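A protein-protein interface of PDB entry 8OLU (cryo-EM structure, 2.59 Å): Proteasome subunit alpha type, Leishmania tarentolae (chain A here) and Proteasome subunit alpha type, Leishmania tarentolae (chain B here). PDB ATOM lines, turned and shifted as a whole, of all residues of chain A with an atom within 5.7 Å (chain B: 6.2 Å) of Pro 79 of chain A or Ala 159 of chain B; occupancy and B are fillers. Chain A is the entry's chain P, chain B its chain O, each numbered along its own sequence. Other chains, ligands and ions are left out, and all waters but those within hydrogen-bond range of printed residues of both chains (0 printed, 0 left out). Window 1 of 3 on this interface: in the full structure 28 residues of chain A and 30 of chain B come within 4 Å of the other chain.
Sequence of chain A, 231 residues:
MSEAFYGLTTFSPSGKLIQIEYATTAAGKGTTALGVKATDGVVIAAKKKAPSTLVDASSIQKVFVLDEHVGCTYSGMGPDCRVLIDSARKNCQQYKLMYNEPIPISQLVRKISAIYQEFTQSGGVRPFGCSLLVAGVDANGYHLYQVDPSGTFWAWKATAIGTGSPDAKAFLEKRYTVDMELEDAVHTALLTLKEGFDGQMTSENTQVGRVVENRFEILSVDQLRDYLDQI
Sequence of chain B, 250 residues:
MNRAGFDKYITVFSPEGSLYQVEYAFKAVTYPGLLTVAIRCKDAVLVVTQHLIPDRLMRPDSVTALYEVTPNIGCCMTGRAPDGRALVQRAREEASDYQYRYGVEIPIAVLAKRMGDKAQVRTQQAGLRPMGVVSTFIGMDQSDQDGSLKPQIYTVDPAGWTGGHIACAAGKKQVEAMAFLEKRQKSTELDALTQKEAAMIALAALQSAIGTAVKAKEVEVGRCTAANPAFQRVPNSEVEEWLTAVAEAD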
ATOM      1  N   TYR A  74       7.651  18.464  11.236  1.00  0.00           N
ATOM      2  CA  TYR A  74       8.330  17.553  12.106  1.00  0.00           C
ATOM      3  C   TYR A  74       9.281  16.726  11.296  1.00  0.00           C
ATOM      4  O   TYR A  74       9.147  16.551  10.104  1.00  0.00           O
ATOM      5  CB  TYR A  74       7.355  16.600  12.767  1.00  0.00           C
ATOM      6  CG  TYR A  74       6.898  15.503  11.844  1.00  0.00           C
ATOM      7  CD1 TYR A  74       7.618  14.331  11.695  1.00  0.00           C
ATOM      8  CD2 TYR A  74       5.758  15.631  11.085  1.00  0.00           C
ATOM      9  CE1 TYR A  74       7.247  13.333  10.798  1.00  0.00           C
ATOM     10  CE2 TYR A  74       5.366  14.630  10.194  1.00  0.00           C
ATOM     11  CZ  TYR A  74       6.115  13.473  10.023  1.00  0.00           C
ATOM     12  OH  TYR A  74       5.724  12.465   9.156  1.00  0.00           O
ATOM     13  N   MET A  77      10.044  10.151  13.269  1.00  0.00           N
ATOM     14  CA  MET A  77       9.021   9.153  13.105  1.00  0.00           C
ATOM     15  C   MET A  77       7.650   9.815  13.056  1.00  0.00           C
ATOM     16  O   MET A  77       7.162  10.375  14.032  1.00  0.00           O
ATOM     17  CB  MET A  77       9.057   8.158  14.255  1.00  0.00           C
ATOM     18  CG  MET A  77      10.401   7.538  14.495  1.00  0.00           C
ATOM     19  SD  MET A  77      10.111   6.392  15.884  1.00  0.00           S
ATOM     20  CE  MET A  77      10.863   4.971  15.065  1.00  0.00           C
ATOM     21  N   GLY A  78       7.003   9.655  11.910  1.00  0.00           N
ATOM     22  CA  GLY A  78       5.708  10.275  11.683  1.00  0.00           C
ATOM     23  C   GLY A  78       4.688  10.027  12.794  1.00  0.00           C
ATOM     24  O   GLY A  78       4.021  10.937  13.260  1.00  0.00           O
ATOM     25  N   PRO A  79       4.440   8.762  13.117  1.00  0.00           N
ATOM     26  CA  PRO A  79       3.352   8.408  14.003  1.00  0.00           C
ATOM     27  C   PRO A  79       3.598   8.829  15.431  1.00  0.00           C
ATOM     28  O   PRO A  79       2.665   8.913  16.218  1.00  0.00           O
ATOM     29  CB  PRO A  79       3.331   6.879  13.925  1.00  0.00           C
ATOM     30  CG  PRO A  79       4.071   6.553  12.677  1.00  0.00           C
ATOM     31  CD  PRO A  79       5.153   7.599  12.586  1.00  0.00           C
ATOM     32  N   ASP A  80       4.869   9.004  15.791  1.00  0.00           N
ATOM     33  CA  ASP A  80       5.191   9.480  17.114  1.00  0.00           C
ATOM     34  C   ASP A  80       4.778  10.941  17.132  1.00  0.00           C
ATOM     35  O   ASP A  80       4.112  11.430  18.029  1.00  0.00           O
ATOM     36  CB  ASP A  80       6.681   9.341  17.424  1.00  0.00           C
ATOM     37  CG  ASP A  80       7.168   8.014  18.009  1.00  0.00           C
ATOM     38  OD1 ASP A  80       6.363   7.037  18.116  1.00  0.00           O
ATOM     39  OD2 ASP A  80       8.383   7.970  18.352  1.00  0.00           O
ATOM     40  N   CYS A  81       5.141  11.625  16.079  1.00  0.00           N
ATOM     41  CA  CYS A  81       4.769  13.011  15.962  1.00  0.00           C
ATOM     42  C   CYS A  81       3.261  13.216  15.938  1.00  0.00           C
ATOM     43  O   CYS A  81       2.751  14.186  16.462  1.00  0.00           O
ATOM     44  CB  CYS A  81       5.372  13.511  14.676  1.00  0.00           C
ATOM     45  SG  CYS A  81       5.082  15.262  14.446  1.00  0.00           S
ATOM     46  N   ARG A  82       2.527  12.293  15.349  1.00  0.00           N
ATOM     47  CA  ARG A  82       1.086  12.392  15.305  1.00  0.00           C
ATOM     48  C   ARG A  82       0.574  12.426  16.743  1.00  0.00           C
ATOM     49  O   ARG A  82      -0.315  13.215  17.068  1.00  0.00           O
ATOM     50  CB  ARG A  82       0.563  11.304  14.363  1.00  0.00           C
ATOM     51  CG  ARG A  82      -0.907  11.410  13.991  1.00  0.00           C
ATOM     52  CD  ARG A  82      -1.375  12.871  14.161  1.00  0.00           C
ATOM     53  NE  ARG A  82      -2.619  13.343  13.548  1.00  0.00           N
ATOM     54  CZ  ARG A  82      -2.865  13.364  12.241  1.00  0.00           C
ATOM     55  NH1 ARG A  82      -2.036  12.777  11.371  1.00  0.00           N
ATOM     56  NH2 ARG A  82      -4.000  13.931  11.853  1.00  0.00           N
ATOM     57  N   VAL A  83       1.215  11.680  17.655  1.00  0.00           N
ATOM     58  CA  VAL A  83       0.847  11.743  19.063  1.00  0.00           C
ATOM     59  C   VAL A  83       1.003  13.141  19.605  1.00  0.00           C
ATOM     60  O   VAL A  83       0.192  13.568  20.415  1.00  0.00           O
ATOM     61  CB  VAL A  83       1.685  10.777  19.917  1.00  0.00           C
ATOM     62  CG1 VAL A  83       1.453  10.922  21.411  1.00  0.00           C
ATOM     63  CG2 VAL A  83       1.419   9.352  19.553  1.00  0.00           C
ATOM     64  N   VAL B  22       9.315  -3.269  15.716  1.00  0.00           N
ATOM     65  CA  VAL B  22       8.472  -2.788  14.630  1.00  0.00           C
ATOM     66  C   VAL B  22       8.947  -3.285  13.303  1.00  0.00           C
ATOM     67  O   VAL B  22       8.115  -3.650  12.529  1.00  0.00           O
ATOM     68  CB  VAL B  22       8.345  -1.257  14.609  1.00  0.00           C
ATOM     69  CG1 VAL B  22       7.607  -0.793  13.395  1.00  0.00           C
ATOM     70  CG2 VAL B  22       7.636  -0.749  15.855  1.00  0.00           C
ATOM     71  N   PHE B  26       6.934  -5.974  10.655  1.00  0.00           N
ATOM     72  CA  PHE B  26       6.744  -5.900   9.217  1.00  0.00           C
ATOM     73  C   PHE B  26       7.047  -7.212   8.544  1.00  0.00           C
ATOM     74  O   PHE B  26       6.582  -7.431   7.457  1.00  0.00           O
ATOM     75  CB  PHE B  26       7.659  -4.870   8.577  1.00  0.00           C
ATOM     76  CG  PHE B  26       7.019  -3.512   8.457  1.00  0.00           C
ATOM     77  CD1 PHE B  26       6.144  -3.240   7.409  1.00  0.00           C
ATOM     78  CD2 PHE B  26       7.225  -2.547   9.426  1.00  0.00           C
ATOM     79  CE1 PHE B  26       5.520  -2.006   7.320  1.00  0.00           C
ATOM     80  CE2 PHE B  26       6.607  -1.316   9.341  1.00  0.00           C
ATOM     81  CZ  PHE B  26       5.767  -1.045   8.282  1.00  0.00           C
ATOM     82  N   GLY B 116      -3.904   4.027  13.171  1.00  0.00           N
ATOM     83  CA  GLY B 116      -2.495   4.304  13.270  1.00  0.00           C
ATOM     84  C   GLY B 116      -2.102   4.773  14.656  1.00  0.00           C
ATOM     85  O   GLY B 116      -1.002   4.511  15.088  1.00  0.00           O
ATOM     86  N   ASP B 117      -2.978   5.501  15.328  1.00  0.00           N
ATOM     87  CA  ASP B 117      -2.669   5.926  16.666  1.00  0.00           C
ATOM     88  C   ASP B 117      -2.553   4.722  17.580  1.00  0.00           C
ATOM     89  O   ASP B 117      -1.717   4.702  18.464  1.00  0.00           O
ATOM     90  CB  ASP B 117      -3.734   6.835  17.247  1.00  0.00           C
ATOM     91  CG  ASP B 117      -3.850   8.279  16.739  1.00  0.00           C
ATOM     92  OD1 ASP B 117      -2.872   8.805  16.063  1.00  0.00           O
ATOM     93  OD2 ASP B 117      -4.987   8.900  16.993  1.00  0.00           O
ATOM     94  N   ALA B 119      -1.809   1.686  16.728  1.00  0.00           N
ATOM     95  CA  ALA B 119      -0.613   0.924  16.509  1.00  0.00           C
ATOM     96  C   ALA B 119       0.589   1.628  17.132  1.00  0.00           C
ATOM     97  O   ALA B 119       1.469   1.008  17.691  1.00  0.00           O
ATOM     98  CB  ALA B 119      -0.399   0.734  15.031  1.00  0.00           C
ATOM     99  N   GLN B 120       0.729   2.909  16.865  1.00  0.00           N
ATOM    100  CA  GLN B 120       1.836   3.674  17.375  1.00  0.00           C
ATOM    101  C   GLN B 120       2.011   3.392  18.853  1.00  0.00           C
ATOM    102  O   GLN B 120       3.145   3.307  19.315  1.00  0.00           O
ATOM    103  CB  GLN B 120       1.583   5.180  17.240  1.00  0.00           C
ATOM    104  CG  GLN B 120       2.782   6.029  17.629  1.00  0.00           C
ATOM    105  CD  GLN B 120       2.933   6.296  19.099  1.00  0.00           C
ATOM    106  OE1 GLN B 120       1.980   6.272  19.899  1.00  0.00           O
ATOM    107  NE2 GLN B 120       4.157   6.643  19.449  1.00  0.00           N
ATOM    108  N   THR B 123       3.945   0.627  19.854  1.00  0.00           N
ATOM    109  CA  THR B 123       5.381   0.716  19.612  1.00  0.00           C
ATOM    110  C   THR B 123       6.100   1.595  20.640  1.00  0.00           C
ATOM    111  O   THR B 123       7.290   1.844  20.543  1.00  0.00           O
ATOM    112  CB  THR B 123       5.666   1.374  18.276  1.00  0.00           C
ATOM    113  OG1 THR B 123       5.404   2.773  18.255  1.00  0.00           O
ATOM    114  CG2 THR B 123       4.796   0.809  17.200  1.00  0.00           C
ATOM    115  N   ASP B 157       0.188   0.544   8.908  1.00  0.00           N
ATOM    116  CA  ASP B 157       1.148  -0.508   9.055  1.00  0.00           C
ATOM    117  C   ASP B 157       1.504  -0.668  10.521  1.00  0.00           C
ATOM    118  O   ASP B 157       1.013   0.025  11.409  1.00  0.00           O
ATOM    119  CB  ASP B 157       2.303  -0.186   8.134  1.00  0.00           C
ATOM    120  CG  ASP B 157       3.088   1.019   8.618  1.00  0.00           C
ATOM    121  OD1 ASP B 157       3.795   1.668   7.763  1.00  0.00           O
ATOM    122  OD2 ASP B 157       3.088   1.245   9.849  1.00  0.00           O
ATOM    123  N   PRO B 158       2.318  -1.649  10.874  1.00  0.00           N
ATOM    124  CA  PRO B 158       2.570  -1.914  12.284  1.00  0.00           C
ATOM    125  C   PRO B 158       3.269  -0.789  13.046  1.00  0.00           C
ATOM    126  O   PRO B 158       3.120  -0.700  14.265  1.00  0.00           O
ATOM    127  CB  PRO B 158       3.472  -3.128  12.232  1.00  0.00           C
ATOM    128  CG  PRO B 158       3.045  -3.772  10.923  1.00  0.00           C
ATOM    129  CD  PRO B 158       2.935  -2.602   9.970  1.00  0.00           C
ATOM    130  N   ALA B 159       3.980   0.092  12.349  1.00  0.00           N
ATOM    131  CA  ALA B 159       4.557   1.258  12.993  1.00  0.00           C
ATOM    132  C   ALA B 159       3.530   2.325  13.312  1.00  0.00           C
ATOM    133  O   ALA B 159       3.861   3.306  13.955  1.00  0.00           O
ATOM    134  CB  ALA B 159       5.543   1.887  12.038  1.00  0.00           C
ATOM    135  N   GLY B 160       2.365   2.242  12.686  1.00  0.00           N
ATOM    136  CA  GLY B 160       1.349   3.253  12.845  1.00  0.00           C
ATOM    137  C   GLY B 160       1.370   4.260  11.718  1.00  0.00           C
ATOM    138  O   GLY B 160       0.664   5.285  11.791  1.00  0.00           O
ATOM    139  N   TRP B 161       2.181   3.978  10.707  1.00  0.00           N
ATOM    140  CA  TRP B 161       2.258   4.890   9.594  1.00  0.00           C
ATOM    141  C   TRP B 161       1.029   4.700   8.731  1.00  0.00           C
ATOM    142  O   TRP B 161       0.725   3.627   8.262  1.00  0.00           O
ATOM    143  CB  TRP B 161       3.545   4.738   8.825  1.00  0.00           C
ATOM    144  CG  TRP B 161       3.652   5.750   7.731  1.00  0.00           C
ATOM    145  CD1 TRP B 161       4.164   7.018   7.815  1.00  0.00           C
ATOM    146  CD2 TRP B 161       3.183   5.591   6.386  1.00  0.00           C
ATOM    147  NE1 TRP B 161       4.034   7.663   6.613  1.00  0.00           N
ATOM    148  CE2 TRP B 161       3.449   6.806   5.712  1.00  0.00           C
ATOM    149  CE3 TRP B 161       2.542   4.551   5.690  1.00  0.00           C
ATOM    150  CZ2 TRP B 161       3.111   6.991   4.363  1.00  0.00           C
ATOM    151  CZ3 TRP B 161       2.213   4.734   4.358  1.00  0.00           C
ATOM    152  CH2 TRP B 161       2.499   5.941   3.703  1.00  0.00           C
ATOM    153  N   THR B 162       0.275   5.752   8.550  1.00  0.00           N
ATOM    154  CA  THR B 162      -0.998   5.695   7.870  1.00  0.00           C
ATOM    155  C   THR B 162      -0.789   6.394   6.553  1.00  0.00           C
ATOM    156  O   THR B 162      -0.096   7.390   6.493  1.00  0.00           O
ATOM    157  CB  THR B 162      -2.016   6.447   8.736  1.00  0.00           C
ATOM    158  OG1 THR B 162      -2.436   5.684   9.881  1.00  0.00           O
ATOM    159  CG2 THR B 162      -3.205   6.897   7.925  1.00  0.00           C
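The side-chain hydroxyl of Thr 123 of chain B is in hydrogen-bond range of the backbone carbonyl oxygen of Gln 120 of chain B, 2.6 Å away. The side-chain carboxylate (OD2) of Asp 157 of chain B lies within hydrogen-bond range of the backbone NH (N) of Ala 159 of chain B (2.9 Å). The backbone NH (N) of Gly 160 of chain B sits at hydrogen-bond distance from the side-chain carboxylate (OD2) of Asp 157 of chain B. OD2 of Asp 157 of chain B is in hydrogen-bond range of N of Trp 161 of chain B (3.0 Å).
Printed residues of chain A that touch a printed residue of chain B: Pro 79, Asp 80, Arg 82 and Val 83. Of the 13 printed residues of chain B, 5 touch a printed residue of chain A. Printed residues of chain B that touch a printed residue of chain A: Asp 117, Gln 120, Ala 159, Gly 160 and Trp 161. Among the printed residues, 7 pairs touch across the chains.
Of chain B, only Gln 120 (3.2 Å), Ala 159 (3.5 Å), Gly 160 (3.7 Å) and Trp 161 (3.8 Å) come within 4 Å of Pro 79 of chain A. Printed residues of chain B within 4 Å of Asp 80 of chain A: Gln 120. Ala 159 of chain B touches just one residue of chain A: Pro 79. Of the printed residues of chain A, Trp 161 of chain B touches Pro 79 (3.8 Å). The nearest printed residue of chain A that does not touch Ala 159 of chain B is Asp 80 of chain A (6.1 Å).
Among the printed residues, pairs that only touch across the chains: Val 83 of chain A with Gln 120 of chain B, Pro 79 of chain A with Gln 120 of chain B, Pro 79 of chain A with Ala 159 of chain B, Pro 79 of chain A with Gly 160 of chain B, Pro 79 of chain A with Trp 161 of chain B and Arg 82 of chain A with Asp 117 of chain B.
The side-chain carboxylate of Asp 80 of chain A sits at hydrogen-bond distance from the side-chain amide nitrogen of Gln 120 of chain B (2.6 Å).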
